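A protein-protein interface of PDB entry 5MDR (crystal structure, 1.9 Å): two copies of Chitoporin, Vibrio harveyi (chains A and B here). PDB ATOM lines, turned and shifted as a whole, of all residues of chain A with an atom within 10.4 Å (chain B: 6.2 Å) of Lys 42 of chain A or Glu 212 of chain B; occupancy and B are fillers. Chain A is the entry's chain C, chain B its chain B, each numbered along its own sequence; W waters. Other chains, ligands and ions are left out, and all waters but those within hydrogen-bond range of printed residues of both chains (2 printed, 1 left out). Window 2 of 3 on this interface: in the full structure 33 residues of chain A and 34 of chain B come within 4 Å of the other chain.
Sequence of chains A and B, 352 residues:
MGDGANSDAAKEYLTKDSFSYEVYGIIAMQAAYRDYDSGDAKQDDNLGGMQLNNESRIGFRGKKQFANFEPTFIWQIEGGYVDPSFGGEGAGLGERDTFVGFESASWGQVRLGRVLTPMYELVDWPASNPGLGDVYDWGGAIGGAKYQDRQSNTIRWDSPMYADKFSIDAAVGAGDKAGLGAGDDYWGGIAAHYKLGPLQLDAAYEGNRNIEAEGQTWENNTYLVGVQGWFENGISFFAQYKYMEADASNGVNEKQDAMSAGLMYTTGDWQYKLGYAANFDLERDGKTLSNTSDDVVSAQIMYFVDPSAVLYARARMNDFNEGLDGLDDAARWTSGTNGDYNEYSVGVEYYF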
ATOM      1  N   TYR A  36      18.315  15.136  -6.841  1.00  0.00           N
ATOM      2  CA  TYR A  36      18.833  13.803  -6.525  1.00  0.00           C
ATOM      3  C   TYR A  36      20.056  13.877  -5.630  1.00  0.00           C
ATOM      4  O   TYR A  36      20.843  14.821  -5.696  1.00  0.00           O
ATOM      5  CB  TYR A  36      19.199  13.010  -7.813  1.00  0.00           C
ATOM      6  CG  TYR A  36      18.031  12.342  -8.469  1.00  0.00           C
ATOM      7  CD1 TYR A  36      17.140  13.075  -9.256  1.00  0.00           C
ATOM      8  CD2 TYR A  36      17.785  10.983  -8.288  1.00  0.00           C
ATOM      9  CE1 TYR A  36      16.051  12.478  -9.844  1.00  0.00           C
ATOM     10  CE2 TYR A  36      16.700  10.366  -8.881  1.00  0.00           C
ATOM     11  CZ  TYR A  36      15.825  11.117  -9.660  1.00  0.00           C
ATOM     12  OH  TYR A  36      14.743  10.521 -10.255  1.00  0.00           O
ATOM     13  N   ASP A  37      20.232  12.845  -4.814  1.00  0.00           N
ATOM     14  CA  ASP A  37      21.455  12.674  -4.064  1.00  0.00           C
ATOM     15  C   ASP A  37      21.879  11.218  -4.172  1.00  0.00           C
ATOM     16  O   ASP A  37      21.710  10.422  -3.238  1.00  0.00           O
ATOM     17  CB  ASP A  37      21.231  13.110  -2.610  1.00  0.00           C
ATOM     18  CG  ASP A  37      22.486  13.050  -1.776  1.00  0.00           C
ATOM     19  OD1 ASP A  37      23.613  13.079  -2.314  1.00  0.00           O
ATOM     20  OD2 ASP A  37      22.342  13.015  -0.548  1.00  0.00           O
ATOM     21  N   SER A  38      22.415  10.873  -5.331  1.00  0.00           N
ATOM     22  CA  SER A  38      22.724   9.499  -5.655  1.00  0.00           C
ATOM     23  C   SER A  38      24.102   9.077  -5.145  1.00  0.00           C
ATOM     24  O   SER A  38      24.376   7.899  -5.135  1.00  0.00           O
ATOM     25  CB  SER A  38      22.687   9.290  -7.168  1.00  0.00           C
ATOM     26  OG  SER A  38      23.742  10.012  -7.788  1.00  0.00           O
ATOM     27  N   GLY A  39      24.953  10.015  -4.736  1.00  0.00           N
ATOM     28  CA  GLY A  39      26.372   9.732  -4.521  1.00  0.00           C
ATOM     29  C   GLY A  39      27.267  10.022  -5.732  1.00  0.00           C
ATOM     30  O   GLY A  39      28.477   9.997  -5.608  1.00  0.00           O
ATOM     31  N   ASP A  40      26.683  10.296  -6.902  1.00  0.00           N
ATOM     32  CA  ASP A  40      27.439  10.619  -8.123  1.00  0.00           C
ATOM     33  C   ASP A  40      26.874  11.942  -8.653  1.00  0.00           C
ATOM     34  O   ASP A  40      25.702  12.011  -9.050  1.00  0.00           O
ATOM     35  CB  ASP A  40      27.260   9.449  -9.086  1.00  0.00           C
ATOM     36  CG  ASP A  40      27.768   9.715 -10.504  1.00  0.00           C
ATOM     37  OD1 ASP A  40      28.071  10.845 -10.929  1.00  0.00           O
ATOM     38  OD2 ASP A  40      27.751   8.734 -11.262  1.00  0.00           O
ATOM     39  N   ALA A  41      27.698  12.980  -8.618  1.00  0.00           N
ATOM     40  CA  ALA A  41      27.273  14.353  -8.922  1.00  0.00           C
ATOM     41  C   ALA A  41      26.765  14.499 -10.381  1.00  0.00           C
ATOM     42  O   ALA A  41      25.761  15.167 -10.628  1.00  0.00           O
ATOM     43  CB  ALA A  41      28.409  15.329  -8.652  1.00  0.00           C
ATOM     44  N   LYS A  42      27.399  13.793 -11.307  1.00  0.00           N
ATOM     45  CA  LYS A  42      26.988  13.818 -12.711  1.00  0.00           C
ATOM     46  C   LYS A  42      25.625  13.157 -12.909  1.00  0.00           C
ATOM     47  O   LYS A  42      24.733  13.708 -13.575  1.00  0.00           O
ATOM     48  CB  LYS A  42      28.069  13.180 -13.605  1.00  0.00           C
ATOM     49  CG  LYS A  42      27.737  13.163 -15.095  1.00  0.00           C
ATOM     50  CD  LYS A  42      27.476  14.574 -15.636  1.00  0.00           C
ATOM     51  CE  LYS A  42      27.372  14.627 -17.172  1.00  0.00           C
ATOM     52  NZ  LYS A  42      26.203  15.467 -17.593  1.00  0.00           N
ATOM     53  N   GLN A  43      25.443  11.989 -12.294  1.00  0.00           N
ATOM     54  CA  GLN A  43      24.144  11.324 -12.312  1.00  0.00           C
ATOM     55  C   GLN A  43      23.060  12.226 -11.697  1.00  0.00           C
ATOM     56  O   GLN A  43      21.966  12.301 -12.230  1.00  0.00           O
ATOM     57  CB  GLN A  43      24.216   9.976 -11.588  1.00  0.00           C
ATOM     58  CG  GLN A  43      22.925   9.163 -11.594  1.00  0.00           C
ATOM     59  CD  GLN A  43      23.049   7.867 -10.778  1.00  0.00           C
ATOM     60  OE1 GLN A  43      24.099   7.229 -10.794  1.00  0.00           O
ATOM     61  NE2 GLN A  43      21.999   7.489 -10.059  1.00  0.00           N
ATOM     62  N   ASP A  44      23.388  12.918 -10.610  1.00  0.00           N
ATOM     63  CA  ASP A  44      22.441  13.882 -10.018  1.00  0.00           C
ATOM     64  C   ASP A  44      22.040  14.994 -11.002  1.00  0.00           C
ATOM     65  O   ASP A  44      20.861  15.315 -11.136  1.00  0.00           O
ATOM     66  CB  ASP A  44      23.012  14.527  -8.762  1.00  0.00           C
ATOM     67  CG  ASP A  44      23.235  13.535  -7.625  1.00  0.00           C
ATOM     68  OD1 ASP A  44      22.686  12.411  -7.617  1.00  0.00           O
ATOM     69  OD2 ASP A  44      23.953  13.925  -6.700  1.00  0.00           O
ATOM     70  N   ASP A  45      23.022  15.534 -11.704  1.00  0.00           N
ATOM     71  CA  ASP A  45      22.783  16.566 -12.717  1.00  0.00           C
ATOM     72  C   ASP A  45      21.906  16.020 -13.821  1.00  0.00           C
ATOM     73  O   ASP A  45      21.003  16.724 -14.301  1.00  0.00           O
ATOM     74  CB  ASP A  45      24.080  17.051 -13.362  1.00  0.00           C
ATOM     75  CG  ASP A  45      24.976  17.801 -12.427  1.00  0.00           C
ATOM     76  OD1 ASP A  45      24.522  18.263 -11.362  1.00  0.00           O
ATOM     77  OD2 ASP A  45      26.158  17.940 -12.793  1.00  0.00           O
ATOM     78  N   ASN A  46      22.168  14.781 -14.237  1.00  0.00           N
ATOM     79  CA  ASN A  46      21.428  14.176 -15.332  1.00  0.00           C
ATOM     80  C   ASN A  46      19.971  13.862 -14.984  1.00  0.00           C
ATOM     81  O   ASN A  46      19.039  14.310 -15.687  1.00  0.00           O
ATOM     82  CB  ASN A  46      22.109  12.908 -15.820  1.00  0.00           C
ATOM     83  CG  ASN A  46      23.434  13.175 -16.518  1.00  0.00           C
ATOM     84  OD1 ASN A  46      23.823  14.307 -16.784  1.00  0.00           O
ATOM     85  ND2 ASN A  46      24.134  12.101 -16.819  1.00  0.00           N
ATOM     86  N   LEU A  47      19.760  13.138 -13.885  1.00  0.00           N
ATOM     87  CA  LEU A  47      18.404  12.746 -13.480  1.00  0.00           C
ATOM     88  C   LEU A  47      17.568  13.904 -12.937  1.00  0.00           C
ATOM     89  O   LEU A  47      16.364  13.891 -13.073  1.00  0.00           O
ATOM     90  CB  LEU A  47      18.461  11.647 -12.422  1.00  0.00           C
ATOM     91  CG  LEU A  47      19.029  10.303 -12.920  1.00  0.00           C
ATOM     92  CD1 LEU A  47      19.276   9.404 -11.734  1.00  0.00           C
ATOM     93  CD2 LEU A  47      18.070   9.634 -13.867  1.00  0.00           C
ATOM     94  N   GLY A  48      18.225  14.857 -12.286  1.00  0.00           N
ATOM     95  CA  GLY A  48      17.569  16.001 -11.656  1.00  0.00           C
ATOM     96  C   GLY A  48      17.311  17.171 -12.596  1.00  0.00           C
ATOM     97  O   GLY A  48      17.673  17.110 -13.788  1.00  0.00           O
ATOM     98  N   GLY A  49      16.745  18.238 -12.039  1.00  0.00           N
ATOM     99  CA  GLY A  49      16.350  19.419 -12.803  1.00  0.00           C
ATOM    100  C   GLY A  49      14.847  19.435 -13.076  1.00  0.00           C
ATOM    101  O   GLY A  49      14.090  18.584 -12.573  1.00  0.00           O
ATOM    102  N   ASN A 338      18.401   4.366  -8.975  1.00  0.00           N
ATOM    103  CA  ASN A 338      18.849   5.692  -9.394  1.00  0.00           C
ATOM    104  C   ASN A 338      19.169   6.705  -8.277  1.00  0.00           C
ATOM    105  O   ASN A 338      19.675   7.786  -8.579  1.00  0.00           O
ATOM    106  CB  ASN A 338      17.805   6.293 -10.345  1.00  0.00           C
ATOM    107  CG  ASN A 338      17.747   5.597 -11.690  1.00  0.00           C
ATOM    108  OD1 ASN A 338      16.767   5.725 -12.387  1.00  0.00           O
ATOM    109  ND2 ASN A 338      18.773   4.887 -12.059  1.00  0.00           N
ATOM    110  N   LYS B 177      18.819  15.756 -23.934  1.00  0.00           N
ATOM    111  CA  LYS B 177      19.268  14.770 -22.946  1.00  0.00           C
ATOM    112  C   LYS B 177      18.538  14.938 -21.612  1.00  0.00           C
ATOM    113  O   LYS B 177      18.115  13.945 -21.015  1.00  0.00           O
ATOM    114  CB  LYS B 177      20.765  14.841 -22.742  1.00  0.00           C
ATOM    115  CG  LYS B 177      21.501  14.457 -24.007  1.00  0.00           C
ATOM    116  CD  LYS B 177      22.959  14.261 -23.672  1.00  0.00           C
ATOM    117  CE  LYS B 177      23.719  13.594 -24.802  1.00  0.00           C
ATOM    118  NZ  LYS B 177      24.946  13.062 -24.119  1.00  0.00           N
ATOM    119  N   ALA B 182      19.066  12.347 -18.818  1.00  0.00           N
ATOM    120  CA  ALA B 182      20.380  11.896 -19.262  1.00  0.00           C
ATOM    121  C   ALA B 182      21.351  13.064 -19.461  1.00  0.00           C
ATOM    122  O   ALA B 182      22.418  12.873 -20.008  1.00  0.00           O
ATOM    123  CB  ALA B 182      20.232  11.085 -20.565  1.00  0.00           C
ATOM    124  N   GLY B 183      21.010  14.251 -18.973  1.00  0.00           N
ATOM    125  CA  GLY B 183      21.862  15.408 -19.140  1.00  0.00           C
ATOM    126  C   GLY B 183      21.235  16.610 -18.474  1.00  0.00           C
ATOM    127  O   GLY B 183      20.182  16.482 -17.805  1.00  0.00           O
ATOM    128  N   ASP B 184      21.893  17.754 -18.625  1.00  0.00           N
ATOM    129  CA  ASP B 184      21.447  19.003 -18.010  1.00  0.00           C
ATOM    130  C   ASP B 184      21.495  20.139 -19.002  1.00  0.00           C
ATOM    131  O   ASP B 184      21.686  21.303 -18.635  1.00  0.00           O
ATOM    132  CB  ASP B 184      22.223  19.305 -16.731  1.00  0.00           C
ATOM    133  CG  ASP B 184      23.721  19.420 -16.954  1.00  0.00           C
ATOM    134  OD1 ASP B 184      24.200  19.255 -18.096  1.00  0.00           O
ATOM    135  OD2 ASP B 184      24.432  19.672 -15.970  1.00  0.00           O
ATOM    136  N   ASP B 185      21.308  19.778 -20.275  1.00  0.00           N
ATOM    137  CA  ASP B 185      21.203  20.753 -21.343  1.00  0.00           C
ATOM    138  C   ASP B 185      19.900  21.561 -21.207  1.00  0.00           C
ATOM    139  O   ASP B 185      18.889  21.069 -20.680  1.00  0.00           O
ATOM    140  CB  ASP B 185      21.350  20.114 -22.768  1.00  0.00           C
ATOM    141  CG  ASP B 185      20.588  18.794 -22.960  1.00  0.00           C
ATOM    142  OD1 ASP B 185      19.858  18.317 -22.044  1.00  0.00           O
ATOM    143  OD2 ASP B 185      20.725  18.191 -24.057  1.00  0.00           O
ATOM    144  N   ASN B 210      25.106  23.647 -21.946  1.00  0.00           N
ATOM    145  CA  ASN B 210      25.378  22.325 -21.425  1.00  0.00           C
ATOM    146  C   ASN B 210      25.120  21.223 -22.476  1.00  0.00           C
ATOM    147  O   ASN B 210      24.680  20.114 -22.149  1.00  0.00           O
ATOM    148  CB  ASN B 210      24.555  22.036 -20.150  1.00  0.00           C
ATOM    149  CG  ASN B 210      25.021  22.826 -18.941  1.00  0.00           C
ATOM    150  OD1 ASN B 210      26.066  23.416 -18.941  1.00  0.00           O
ATOM    151  ND2 ASN B 210      24.232  22.802 -17.897  1.00  0.00           N
ATOM    152  N   ILE B 211      25.423  21.531 -23.737  1.00  0.00           N
ATOM    153  CA  ILE B 211      25.198  20.598 -24.836  1.00  0.00           C
ATOM    154  C   ILE B 211      26.371  19.639 -24.900  1.00  0.00           C
ATOM    155  O   ILE B 211      27.509  20.073 -25.035  1.00  0.00           O
ATOM    156  CB  ILE B 211      25.076  21.347 -26.188  1.00  0.00           C
ATOM    157  CG1 ILE B 211      23.896  22.319 -26.163  1.00  0.00           C
ATOM    158  CG2 ILE B 211      24.972  20.375 -27.368  1.00  0.00           C
ATOM    159  CD1 ILE B 211      22.533  21.685 -26.097  1.00  0.00           C
ATOM    160  N   GLU B 212      26.108  18.343 -24.838  1.00  0.00           N
ATOM    161  CA  GLU B 212      27.189  17.356 -24.849  1.00  0.00           C
ATOM    162  C   GLU B 212      27.327  16.746 -26.237  1.00  0.00           C
ATOM    163  O   GLU B 212      26.385  16.181 -26.760  1.00  0.00           O
ATOM    164  CB  GLU B 212      26.939  16.293 -23.783  1.00  0.00           C
ATOM    165  CG  GLU B 212      27.145  16.850 -22.378  1.00  0.00           C
ATOM    166  CD  GLU B 212      26.665  15.911 -21.273  1.00  0.00           C
ATOM    167  OE1 GLU B 212      26.234  14.792 -21.557  1.00  0.00           O
ATOM    168  OE2 GLU B 212      26.694  16.292 -20.100  1.00  0.00           O
ATOM    169  N   ALA B 213      28.492  16.909 -26.854  1.00  0.00           N
ATOM    170  CA  ALA B 213      28.728  16.344 -28.192  1.00  0.00           C
ATOM    171  C   ALA B 213      30.204  16.333 -28.466  1.00  0.00           C
ATOM    172  O   ALA B 213      30.940  17.229 -28.023  1.00  0.00           O
ATOM    173  CB  ALA B 213      28.008  17.152 -29.270  1.00  0.00           C
ATOM    174  N   GLU B 214      30.652  15.283 -29.153  1.00  0.00           N
ATOM    175  CA  GLU B 214      32.044  15.170 -29.625  1.00  0.00           C
ATOM    176  C   GLU B 214      33.062  15.202 -28.491  1.00  0.00           C
ATOM    177  O   GLU B 214      34.187  15.671 -28.659  1.00  0.00           O
ATOM    178  CB  GLU B 214      32.343  16.276 -30.671  1.00  0.00           C
ATOM    179  CG  GLU B 214      31.390  16.244 -31.872  1.00  0.00           C
ATOM    180  CD  GLU B 214      31.544  17.432 -32.831  1.00  0.00           C
ATOM    181  OE1 GLU B 214      32.526  18.219 -32.726  1.00  0.00           O
ATOM    182  OE2 GLU B 214      30.675  17.562 -33.707  1.00  0.00           O
ATOM    183  N   GLY B 215      32.653  14.714 -27.321  1.00  0.00           N
ATOM    184  CA  GLY B 215      33.535  14.687 -26.136  1.00  0.00           C
ATOM    185  C   GLY B 215      33.652  16.009 -25.403  1.00  0.00           C
ATOM    186  O   GLY B 215      34.466  16.134 -24.507  1.00  0.00           O
ATOM    187  N   GLN B 216      32.841  17.010 -25.778  1.00  0.00           N
ATOM    188  CA  GLN B 216      32.906  18.344 -25.171  1.00  0.00           C
ATOM    189  C   GLN B 216      31.522  18.721 -24.661  1.00  0.00           C
ATOM    190  O   GLN B 216      30.529  18.100 -24.984  1.00  0.00           O
ATOM    191  CB  GLN B 216      33.271  19.424 -26.196  1.00  0.00           C
ATOM    192  CG  GLN B 216      34.396  19.104 -27.135  1.00  0.00           C
ATOM    193  CD  GLN B 216      35.659  18.813 -26.398  1.00  0.00           C
ATOM    194  OE1 GLN B 216      36.027  19.497 -25.457  1.00  0.00           O
ATOM    195  NE2 GLN B 216      36.345  17.775 -26.837  1.00  0.00           N
ATOM    196  N   THR B 217      31.505  19.779 -23.862  1.00  0.00           N
ATOM    197  CA  THR B 217      30.304  20.510 -23.524  1.00  0.00           C
ATOM    198  C   THR B 217      30.356  21.819 -24.298  1.00  0.00           C
ATOM    199  O   THR B 217      31.385  22.492 -24.319  1.00  0.00           O
ATOM    200  CB  THR B 217      30.215  20.762 -22.007  1.00  0.00           C
ATOM    201  OG1 THR B 217      30.241  19.494 -21.363  1.00  0.00           O
ATOM    202  CG2 THR B 217      28.873  21.397 -21.640  1.00  0.00           C
ATOM    203  N   TRP B 218      29.230  22.179 -24.900  1.00  0.00           N
ATOM    204  CA  TRP B 218      29.145  23.335 -25.771  1.00  0.00           C
ATOM    205  C   TRP B 218      28.132  24.367 -25.272  1.00  0.00           C
ATOM    206  O   TRP B 218      27.100  24.022 -24.686  1.00  0.00           O
ATOM    207  CB  TRP B 218      28.678  22.911 -27.173  1.00  0.00           C
ATOM    208  CG  TRP B 218      29.542  21.969 -27.906  1.00  0.00           C
ATOM    209  CD1 TRP B 218      29.640  20.611 -27.725  1.00  0.00           C
ATOM    210  CD2 TRP B 218      30.376  22.283 -29.024  1.00  0.00           C
ATOM    211  NE1 TRP B 218      30.519  20.076 -28.636  1.00  0.00           N
ATOM    212  CE2 TRP B 218      30.978  21.073 -29.455  1.00  0.00           C
ATOM    213  CE3 TRP B 218      30.696  23.469 -29.683  1.00  0.00           C
ATOM    214  CZ2 TRP B 218      31.876  21.018 -30.521  1.00  0.00           C
ATOM    215  CZ3 TRP B 218      31.603  23.417 -30.758  1.00  0.00           C
ATOM    216  CH2 TRP B 218      32.184  22.193 -31.159  1.00  0.00           C
HETATM  217  O   HOH W   1      23.086  20.496 -13.618  1.00  0.00           O
HETATM  218  O   HOH W   2      26.605  17.881 -15.625  1.00  0.00           O
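Lys 42 of chain A touches just one residue of chain B: Glu 212.
Printed residues of chain B within 4 Å of Asp 45 of chain A: Gly 183 and Asp 184.
Of the printed residues of chain B, Asn 46 of chain A touches Ala 182 (3.6 Å) and Gly 183 (3.2 Å).
Gly 49 of chain A touches none of the printed residues of chain B.
Gly 183 of chain B touches two residues of chain A.
Of the printed residues of chain A, Asp 184 of chain B touches Asp 45 (3.7 Å).
Ile 211 of chain B touches none of the printed residues of chain A.
Of chain A, only Lys 42 comes within 4 Å of Glu 212 of chain B.
No residue of chain A comes within 4 Å of Ala 213 of chain B.
The nearest residue of chain B that does not touch Lys 42 of chain A is Asp 184 of chain B (4.3 Å).
The nearest residue of chain A that does not touch Glu 212 of chain B is Asn 46 of chain A (4.8 Å).
The backbone NH (N) of Ala 182 of chain B is in hydrogen-bond range of the backbone carbonyl oxygen (O) of Lys 177 of chain B (2.9 Å).
The backbone NH (N) of Lys 42 of chain A lies within hydrogen-bond range of the side-chain carboxylate (OD1) of Asp 40 of chain A, 3.0 Å away.
O of Asp 184 of chain B lies within hydrogen-bond range of ND2 of Asn 210 of chain B, at 3.0 Å.
The side-chain amino group (NZ) of Lys 177 of chain B lies within salt-bridge range of the side-chain carboxylate (OE1) of Glu 212 of chain B (3.3 Å).
NZ of Lys 42 of chain A is in hydrogen-bond range of OD1 of Asn 46 of chain A, at 2.8 Å.
OE2 of Glu 212 of chain B lies within salt-bridge range of NZ of Lys 42 of chain A (2.7 Å).
The backbone carbonyl oxygen (O) of Gly 183 of chain B lies close to the backbone carbonyl oxygen (O) of Asn 46 of chain A.
Among the printed residues, pairs that only touch across the chains: Asp 45 of chain A with Gly 183 of chain B (3.6 Å), Asn 46 of chain A with Ala 182 of chain B (3.6 Å) and Asp 45 of chain A with Asp 184 of chain B (3.7 Å).
Printed residues of chain B that touch a printed residue of chain A: Ala 182, Gly 183, Asp 184 and Glu 212.
Of the 15 printed residues of chain A, 3 touch a printed residue of chain B.
Printed residues of chain A that touch a printed residue of chain B: Lys 42, Asp 45 and Asn 46.
Among the printed residues, 5 pairs touch across the chains.
No position is printed for both chains.
Water W1 lies within hydrogen-bond range of OD2 of Asp 184 of chain B (2.8 Å) and OD1 of Asp 45 of chain A (3.5 Å).
Water W2 lies within hydrogen-bond range of OD2 of Asp 184 of chain B (2.8 Å), OD2 of Asp 45 of chain A (2.9 Å) and NZ of Lys 42 of chain A (3.1 Å).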
